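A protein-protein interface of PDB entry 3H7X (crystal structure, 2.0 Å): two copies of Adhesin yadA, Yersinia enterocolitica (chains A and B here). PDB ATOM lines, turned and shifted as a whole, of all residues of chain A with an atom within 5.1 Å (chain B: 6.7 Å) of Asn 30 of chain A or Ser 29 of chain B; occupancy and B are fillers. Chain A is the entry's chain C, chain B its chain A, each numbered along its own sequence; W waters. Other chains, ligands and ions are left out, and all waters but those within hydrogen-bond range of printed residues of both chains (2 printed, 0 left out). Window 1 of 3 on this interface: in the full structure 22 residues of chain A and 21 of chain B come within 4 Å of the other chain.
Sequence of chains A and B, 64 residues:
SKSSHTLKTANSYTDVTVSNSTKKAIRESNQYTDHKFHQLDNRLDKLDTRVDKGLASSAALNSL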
ATOM      1  N   ALA A  25      15.136  26.984 -23.983  1.00  0.00           N
ATOM      2  CA  ALA A  25      14.493  25.867 -23.345  1.00  0.00           C
ATOM      3  C   ALA A  25      14.283  26.228 -21.849  1.00  0.00           C
ATOM      4  O   ALA A  25      13.183  26.031 -21.292  1.00  0.00           O
ATOM      5  CB  ALA A  25      15.342  24.599 -23.455  1.00  0.00           C
ATOM      6  N   ILE A  26      15.323  26.837 -21.238  1.00  0.00           N
ATOM      7  CA  ILE A  26      15.231  27.366 -19.866  1.00  0.00           C
ATOM      8  C   ILE A  26      14.183  28.532 -19.729  1.00  0.00           C
ATOM      9  O   ILE A  26      13.328  28.563 -18.831  1.00  0.00           O
ATOM     10  CB  ILE A  26      16.653  27.724 -19.337  1.00  0.00           C
ATOM     11  CG1 ILE A  26      17.474  26.463 -19.127  1.00  0.00           C
ATOM     12  CG2 ILE A  26      16.640  28.492 -17.953  1.00  0.00           C
ATOM     13  CD1 ILE A  26      19.093  26.719 -18.882  1.00  0.00           C
ATOM     14  N   ARG A  27      14.161  29.451 -20.672  1.00  0.00           N
ATOM     15  CA  ARG A  27      13.218  30.559 -20.633  1.00  0.00           C
ATOM     16  C   ARG A  27      11.752  30.050 -20.673  1.00  0.00           C
ATOM     17  O   ARG A  27      10.870  30.583 -19.967  1.00  0.00           O
ATOM     18  CB  ARG A  27      13.399  31.554 -21.798  1.00  0.00           C
ATOM     19  CG  ARG A  27      14.752  32.342 -21.903  1.00  0.00           C
ATOM     20  CD  ARG A  27      14.949  32.985 -23.272  1.00  0.00           C
ATOM     21  NE  ARG A  27      16.302  32.801 -23.793  1.00  0.00           N
ATOM     22  CZ  ARG A  27      17.395  33.211 -23.137  1.00  0.00           C
ATOM     23  NH1 ARG A  27      17.280  33.807 -21.948  1.00  0.00           N
ATOM     24  NH2 ARG A  27      18.610  32.986 -23.629  1.00  0.00           N
ATOM     25  N   GLU A  28      11.476  29.120 -21.576  1.00  0.00           N
ATOM     26  CA  GLU A  28      10.149  28.588 -21.746  1.00  0.00           C
ATOM     27  C   GLU A  28       9.759  27.705 -20.546  1.00  0.00           C
ATOM     28  O   GLU A  28       8.653  27.807 -20.089  1.00  0.00           O
ATOM     29  CB  GLU A  28      10.107  27.829 -23.071  1.00  0.00           C
ATOM     30  CG  GLU A  28      10.258  28.778 -24.264  1.00  0.00           C
ATOM     31  CD  GLU A  28       9.560  28.320 -25.474  1.00  0.00           C
ATOM     32  OE1 GLU A  28       8.516  27.596 -25.335  1.00  0.00           O
ATOM     33  OE2 GLU A  28      10.086  28.641 -26.572  1.00  0.00           O
ATOM     34  N   SER A  29      10.636  26.787 -20.114  1.00  0.00           N
ATOM     35  CA  SER A  29      10.376  25.992 -18.902  1.00  0.00           C
ATOM     36  C   SER A  29      10.015  26.924 -17.741  1.00  0.00           C
ATOM     37  O   SER A  29       9.034  26.747 -16.982  1.00  0.00           O
ATOM     38  CB  SER A  29      11.568  25.178 -18.424  1.00  0.00           C
ATOM     39  OG  SER A  29      12.404  24.876 -19.503  1.00  0.00           O
ATOM     40  N   ASN A  30      10.899  27.909 -17.553  1.00  0.00           N
ATOM     41  CA  ASN A  30      10.748  28.758 -16.397  1.00  0.00           C
ATOM     42  C   ASN A  30       9.368  29.583 -16.445  1.00  0.00           C
ATOM     43  O   ASN A  30       8.799  29.772 -15.425  1.00  0.00           O
ATOM     44  CB  ASN A  30      11.928  29.631 -16.289  1.00  0.00           C
ATOM     45  CG  ASN A  30      13.088  29.039 -15.563  1.00  0.00           C
ATOM     46  OD1 ASN A  30      13.323  27.832 -15.398  1.00  0.00           O
ATOM     47  ND2 ASN A  30      13.945  29.965 -15.183  1.00  0.00           N
ATOM     48  N   GLN A  31       8.884  29.981 -17.612  1.00  0.00           N
ATOM     49  CA  GLN A  31       7.644  30.684 -17.819  1.00  0.00           C
ATOM     50  C   GLN A  31       6.484  29.673 -17.554  1.00  0.00           C
ATOM     51  O   GLN A  31       5.465  30.028 -16.977  1.00  0.00           O
ATOM     52  CB  GLN A  31       7.591  31.212 -19.250  1.00  0.00           C
ATOM     53  CG  GLN A  31       6.317  32.100 -19.579  1.00  0.00           C
ATOM     54  CD  GLN A  31       6.282  32.500 -20.982  1.00  0.00           C
ATOM     55  OE1 GLN A  31       7.279  33.021 -21.490  1.00  0.00           O
ATOM     56  NE2 GLN A  31       5.167  32.290 -21.648  1.00  0.00           N
ATOM     57  N   TYR A  32       6.648  28.407 -17.970  1.00  0.00           N
ATOM     58  CA  TYR A  32       5.551  27.438 -17.691  1.00  0.00           C
ATOM     59  C   TYR A  32       5.464  27.274 -16.175  1.00  0.00           C
ATOM     60  O   TYR A  32       4.367  27.214 -15.555  1.00  0.00           O
ATOM     61  CB  TYR A  32       5.778  26.154 -18.395  1.00  0.00           C
ATOM     62  CG  TYR A  32       4.641  25.154 -18.207  1.00  0.00           C
ATOM     63  CD1 TYR A  32       3.389  25.317 -18.822  1.00  0.00           C
ATOM     64  CD2 TYR A  32       4.822  24.041 -17.356  1.00  0.00           C
ATOM     65  CE1 TYR A  32       2.328  24.349 -18.619  1.00  0.00           C
ATOM     66  CE2 TYR A  32       3.752  23.073 -17.135  1.00  0.00           C
ATOM     67  CZ  TYR A  32       2.553  23.236 -17.770  1.00  0.00           C
ATOM     68  OH  TYR A  32       1.517  22.308 -17.568  1.00  0.00           O
ATOM     69  N   THR A  33       6.628  27.403 -15.531  1.00  0.00           N
ATOM     70  CA  THR A  33       6.698  27.121 -14.107  1.00  0.00           C
ATOM     71  C   THR A  33       5.987  28.275 -13.378  1.00  0.00           C
ATOM     72  O   THR A  33       5.123  28.087 -12.472  1.00  0.00           O
ATOM     73  CB  THR A  33       8.174  26.978 -13.592  1.00  0.00           C
ATOM     74  OG1 THR A  33       8.811  25.715 -13.920  1.00  0.00           O
ATOM     75  CG2 THR A  33       8.204  27.077 -12.075  1.00  0.00           C
ATOM     76  N   ASP A  34       6.378  29.496 -13.713  1.00  0.00           N
ATOM     77  CA  ASP A  34       5.678  30.632 -13.247  1.00  0.00           C
ATOM     78  C   ASP A  34       4.139  30.640 -13.414  1.00  0.00           C
ATOM     79  O   ASP A  34       3.379  31.057 -12.509  1.00  0.00           O
ATOM     80  CB  ASP A  34       6.175  31.781 -13.995  1.00  0.00           C
ATOM     81  CG  ASP A  34       7.530  32.183 -13.479  1.00  0.00           C
ATOM     82  OD1 ASP A  34       7.995  31.534 -12.496  1.00  0.00           O
ATOM     83  OD2 ASP A  34       8.079  33.053 -14.115  1.00  0.00           O
ATOM     84  N   LYS B  24      21.447  19.743 -19.304  1.00  0.00           N
ATOM     85  CA  LYS B  24      21.582  20.989 -18.563  1.00  0.00           C
ATOM     86  C   LYS B  24      20.320  21.855 -18.553  1.00  0.00           C
ATOM     87  O   LYS B  24      20.041  22.584 -17.627  1.00  0.00           O
ATOM     88  CB  LYS B  24      22.752  21.824 -19.116  1.00  0.00           C
ATOM     89  CG  LYS B  24      22.727  23.264 -18.778  1.00  0.00           C
ATOM     90  CD  LYS B  24      24.050  23.933 -19.335  1.00  0.00           C
ATOM     91  CE  LYS B  24      23.871  25.506 -19.626  1.00  0.00           C
ATOM     92  NZ  LYS B  24      23.634  26.411 -18.451  1.00  0.00           N
ATOM     93  N   ALA B  25      19.619  21.899 -19.635  1.00  0.00           N
ATOM     94  CA  ALA B  25      18.501  22.837 -19.706  1.00  0.00           C
ATOM     95  C   ALA B  25      17.492  22.249 -18.694  1.00  0.00           C
ATOM     96  O   ALA B  25      16.930  22.998 -17.982  1.00  0.00           O
ATOM     97  CB  ALA B  25      17.947  22.861 -21.130  1.00  0.00           C
ATOM     98  N   ILE B  26      17.453  20.906 -18.547  1.00  0.00           N
ATOM     99  CA  ILE B  26      16.387  20.187 -17.824  1.00  0.00           C
ATOM    100  C   ILE B  26      16.750  20.295 -16.349  1.00  0.00           C
ATOM    101  O   ILE B  26      15.919  20.521 -15.521  1.00  0.00           O
ATOM    102  CB  ILE B  26      16.310  18.689 -18.269  1.00  0.00           C
ATOM    103  CG1 ILE B  26      15.664  18.578 -19.631  1.00  0.00           C
ATOM    104  CG2 ILE B  26      15.631  17.757 -17.265  1.00  0.00           C
ATOM    105  CD1 ILE B  26      15.696  17.075 -20.126  1.00  0.00           C
ATOM    106  N   ARG B  27      18.030  20.161 -16.044  1.00  0.00           N
ATOM    107  CA  ARG B  27      18.506  20.301 -14.702  1.00  0.00           C
ATOM    108  C   ARG B  27      18.212  21.703 -14.145  1.00  0.00           C
ATOM    109  O   ARG B  27      17.812  21.841 -12.953  1.00  0.00           O
ATOM    110  CB  ARG B  27      20.014  19.950 -14.667  1.00  0.00           C
ATOM    111  CG  ARG B  27      20.316  18.422 -14.694  1.00  0.00           C
ATOM    112  CD  ARG B  27      21.750  18.169 -14.292  1.00  0.00           C
ATOM    113  NE  ARG B  27      22.628  18.869 -15.233  1.00  0.00           N
ATOM    114  CZ  ARG B  27      23.193  18.253 -16.267  1.00  0.00           C
ATOM    115  NH1 ARG B  27      23.016  16.954 -16.416  1.00  0.00           N
ATOM    116  NH2 ARG B  27      23.987  18.946 -17.124  1.00  0.00           N
ATOM    117  N   GLU B  28      18.406  22.731 -14.956  1.00  0.00           N
ATOM    118  CA  GLU B  28      18.210  24.104 -14.492  1.00  0.00           C
ATOM    119  C   GLU B  28      16.774  24.421 -14.339  1.00  0.00           C
ATOM    120  O   GLU B  28      16.424  25.119 -13.435  1.00  0.00           O
ATOM    121  CB  GLU B  28      18.774  25.134 -15.449  1.00  0.00           C
ATOM    122  CG  GLU B  28      20.387  24.990 -15.346  1.00  0.00           C
ATOM    123  CD  GLU B  28      21.052  26.318 -15.746  1.00  0.00           C
ATOM    124  OE1 GLU B  28      20.396  27.370 -15.577  1.00  0.00           O
ATOM    125  OE2 GLU B  28      22.226  26.320 -16.192  1.00  0.00           O
ATOM    126  N   SER B  29      15.954  23.843 -15.215  1.00  0.00           N
ATOM    127  CA  SER B  29      14.541  24.153 -15.223  1.00  0.00           C
ATOM    128  C   SER B  29      13.974  23.566 -13.988  1.00  0.00           C
ATOM    129  O   SER B  29      13.389  24.360 -13.221  1.00  0.00           O
ATOM    130  CB  SER B  29      13.908  23.663 -16.491  1.00  0.00           C
ATOM    131  OG  SER B  29      14.359  24.562 -17.510  1.00  0.00           O
ATOM    132  N   ASN B  30      14.312  22.266 -13.722  1.00  0.00           N
ATOM    133  CA  ASN B  30      13.793  21.607 -12.588  1.00  0.00           C
ATOM    134  C   ASN B  30      14.287  22.179 -11.267  1.00  0.00           C
ATOM    135  O   ASN B  30      13.563  22.209 -10.210  1.00  0.00           O
ATOM    136  CB  ASN B  30      14.072  20.139 -12.750  1.00  0.00           C
ATOM    137  CG  ASN B  30      13.269  19.575 -13.912  1.00  0.00           C
ATOM    138  OD1 ASN B  30      12.479  20.327 -14.555  1.00  0.00           O
ATOM    139  ND2 ASN B  30      13.515  18.316 -14.241  1.00  0.00           N
ATOM    140  N   GLN B  31      15.482  22.733 -11.296  1.00  0.00           N
ATOM    141  CA  GLN B  31      15.910  23.497 -10.099  1.00  0.00           C
ATOM    142  C   GLN B  31      15.026  24.658  -9.795  1.00  0.00           C
ATOM    143  O   GLN B  31      14.679  24.821  -8.589  1.00  0.00           O
ATOM    144  CB  GLN B  31      17.336  23.962 -10.193  1.00  0.00           C
ATOM    145  CG  GLN B  31      17.838  24.729  -9.041  1.00  0.00           C
ATOM    146  CD  GLN B  31      19.267  25.082  -9.339  1.00  0.00           C
ATOM    147  OE1 GLN B  31      19.982  24.253  -9.930  1.00  0.00           O
ATOM    148  NE2 GLN B  31      19.653  26.369  -9.099  1.00  0.00           N
ATOM    149  N   TYR B  32      14.636  25.411 -10.807  1.00  0.00           N
ATOM    150  CA  TYR B  32      13.754  26.568 -10.700  1.00  0.00           C
ATOM    151  C   TYR B  32      12.382  26.181 -10.287  1.00  0.00           C
ATOM    152  O   TYR B  32      11.731  26.998  -9.613  1.00  0.00           O
ATOM    153  CB  TYR B  32      13.631  27.297 -12.014  1.00  0.00           C
ATOM    154  CG  TYR B  32      12.680  28.499 -12.054  1.00  0.00           C
ATOM    155  CD1 TYR B  32      13.117  29.743 -11.627  1.00  0.00           C
ATOM    156  CD2 TYR B  32      11.333  28.394 -12.515  1.00  0.00           C
ATOM    157  CE1 TYR B  32      12.394  30.830 -11.726  1.00  0.00           C
ATOM    158  CE2 TYR B  32      10.522  29.594 -12.593  1.00  0.00           C
ATOM    159  CZ  TYR B  32      11.065  30.789 -12.142  1.00  0.00           C
ATOM    160  OH  TYR B  32      10.414  31.963 -12.119  1.00  0.00           O
ATOM    161  N   THR B  33      11.962  24.953 -10.679  1.00  0.00           N
ATOM    162  CA  THR B  33      10.659  24.460 -10.276  1.00  0.00           C
ATOM    163  C   THR B  33      10.721  24.187  -8.774  1.00  0.00           C
ATOM    164  O   THR B  33       9.796  24.558  -8.016  1.00  0.00           O
ATOM    165  CB  THR B  33      10.308  23.202 -11.061  1.00  0.00           C
ATOM    166  OG1 THR B  33       9.996  23.613 -12.358  1.00  0.00           O
ATOM    167  CG2 THR B  33       9.227  22.418 -10.498  1.00  0.00           C
ATOM    168  N   ASP B  34      11.743  23.533  -8.306  1.00  0.00           N
ATOM    169  CA  ASP B  34      11.774  23.091  -6.927  1.00  0.00           C
ATOM    170  C   ASP B  34      11.786  24.284  -5.969  1.00  0.00           C
ATOM    171  O   ASP B  34      11.050  24.353  -4.982  1.00  0.00           O
ATOM    172  CB  ASP B  34      13.033  22.274  -6.615  1.00  0.00           C
ATOM    173  CG  ASP B  34      12.964  20.900  -7.170  1.00  0.00           C
ATOM    174  OD1 ASP B  34      11.843  20.526  -7.610  1.00  0.00           O
ATOM    175  OD2 ASP B  34      14.037  20.219  -7.212  1.00  0.00           O
HETATM  176  O   HOH W   1      13.115  32.141 -14.190  1.00  0.00           O
HETATM  177  O   HOH W   2      11.560  25.852 -14.289  1.00  0.00           O
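The side-chain hydroxyl (OG1) of Thr 33 of chain A sits at hydrogen-bond distance from the side-chain hydroxyl (OG1) of Thr 33 of chain B, at 2.9 Å.
The side-chain hydroxyl (OG) of Ser 29 of chain B sits at hydrogen-bond distance from the side-chain hydroxyl (OG) of Ser 29 of chain A.
The side-chain hydroxyl (OH) of Tyr 32 of chain B lies within hydrogen-bond range of the side-chain carboxylate (OD1) of Asp 34 of chain A, 2.5 Å away.
Of the 11 printed residues of chain B, 5 touch a printed residue of chain A.
Of the 10 printed residues of chain A, 6 touch a printed residue of chain B.
Hydrophobic or aromatic side chains of chain A that line the printed part of chain B: Ala 25 and Ile 26.
Among the printed residues, 10 pairs touch across the chains.
Water W1 lies within hydrogen-bond range of ND2 of Asn 30 of chain A and OH of Tyr 32 of chain B.
Water W2 lies within hydrogen-bond range of the backbone carbonyl oxygen (O) of Ser 29 of chain B, the side-chain hydroxyl (OG1) of Thr 33 of chain A, the side-chain amide oxygen (OD1) of Asn 30 of chain A and the side-chain hydroxyl (OG1) of Thr 33 of chain B.
Printed residues of chain B within 4 Å of Ala 25 of chain A: Ala 25.
Arg 27 of chain A touches none of the printed residues of chain B.
Of chain B, only Ser 29 (3.9 Å) and Tyr 32 (3.3 Å) come within 4 Å of Asn 30 of chain A.
Gln 31 of chain A touches none of the printed residues of chain B.
Printed residues of chain B within 4 Å of Thr 33 of chain A: Tyr 32 (3.4 Å) and Thr 33 (2.9 Å).
Printed residues of chain A within 4 Å of Glu 28 of chain B: Ile 26.
The nearest residue of chain B that does not touch Asn 30 of chain A is Glu 28 of chain B (4.6 Å).
The nearest residue of chain A that does not touch Ser 29 of chain B is Ala 25 of chain A (4.2 Å).
The nearest printed residue of chain A that does not touch Glu 28 of chain B is Asn 30 of chain A (4.6 Å).
The side-chain hydroxyl of Thr 33 of chain A lies within hydrogen-bond range of the backbone carbonyl oxygen of Ser 29 of chain A (3.2 Å).
The side-chain hydroxyl (OG) of Ser 29 of chain B lies within hydrogen-bond range of the backbone carbonyl oxygen (O) of Ala 25 of chain B, 3.0 Å away.
The side-chain carboxylate (OE2) of Glu 28 of chain B lies within salt-bridge range of the side-chain amino group (NZ) of Lys 24 of chain B, at 2.7 Å.
CB of Ala 25 of chain A touches CB of Ala 25 of chain B, at 3.9 Å.
O of Ala 25 of chain B touches CG1 of Ile 26 of chain A, at 3.7 Å.
Ile 26 of chain A touches Glu 28 of chain B.
Ser 29 of chain B touches Ile 26 of chain A.
Asn 30 of chain A touches Ser 29 of chain B (OD1 to CA, 3.9 Å).
Asn 30 of chain A touches Tyr 32 of chain B.
Tyr 32 of chain B touches Thr 33 of chain A (CD2 to CG2, 3.4 Å).
Ile 26 of chain A touches Glu 28 of chain B, but with the chains exchanged Glu 28 of chain A does not touch Ile 26 of chain B (10.4 Å).
Ser 29 of chain A touches its own counterpart, Ser 29 of chain B.
Thr 33 of chain A touches Tyr 32 of chain B, but with the chains exchanged Tyr 32 of chain A does not touch Thr 33 of chain B (7.0 Å).
Asp 34 of chain A touches Tyr 32 of chain B, but with the chains exchanged Tyr 32 of chain A does not touch Asp 34 of chain B (10.7 Å).
10 positions are printed for both chains.
Of the 10 pairs that touch across the chains among the printed residues, 3 have their exchanged pair printed and touching as well.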
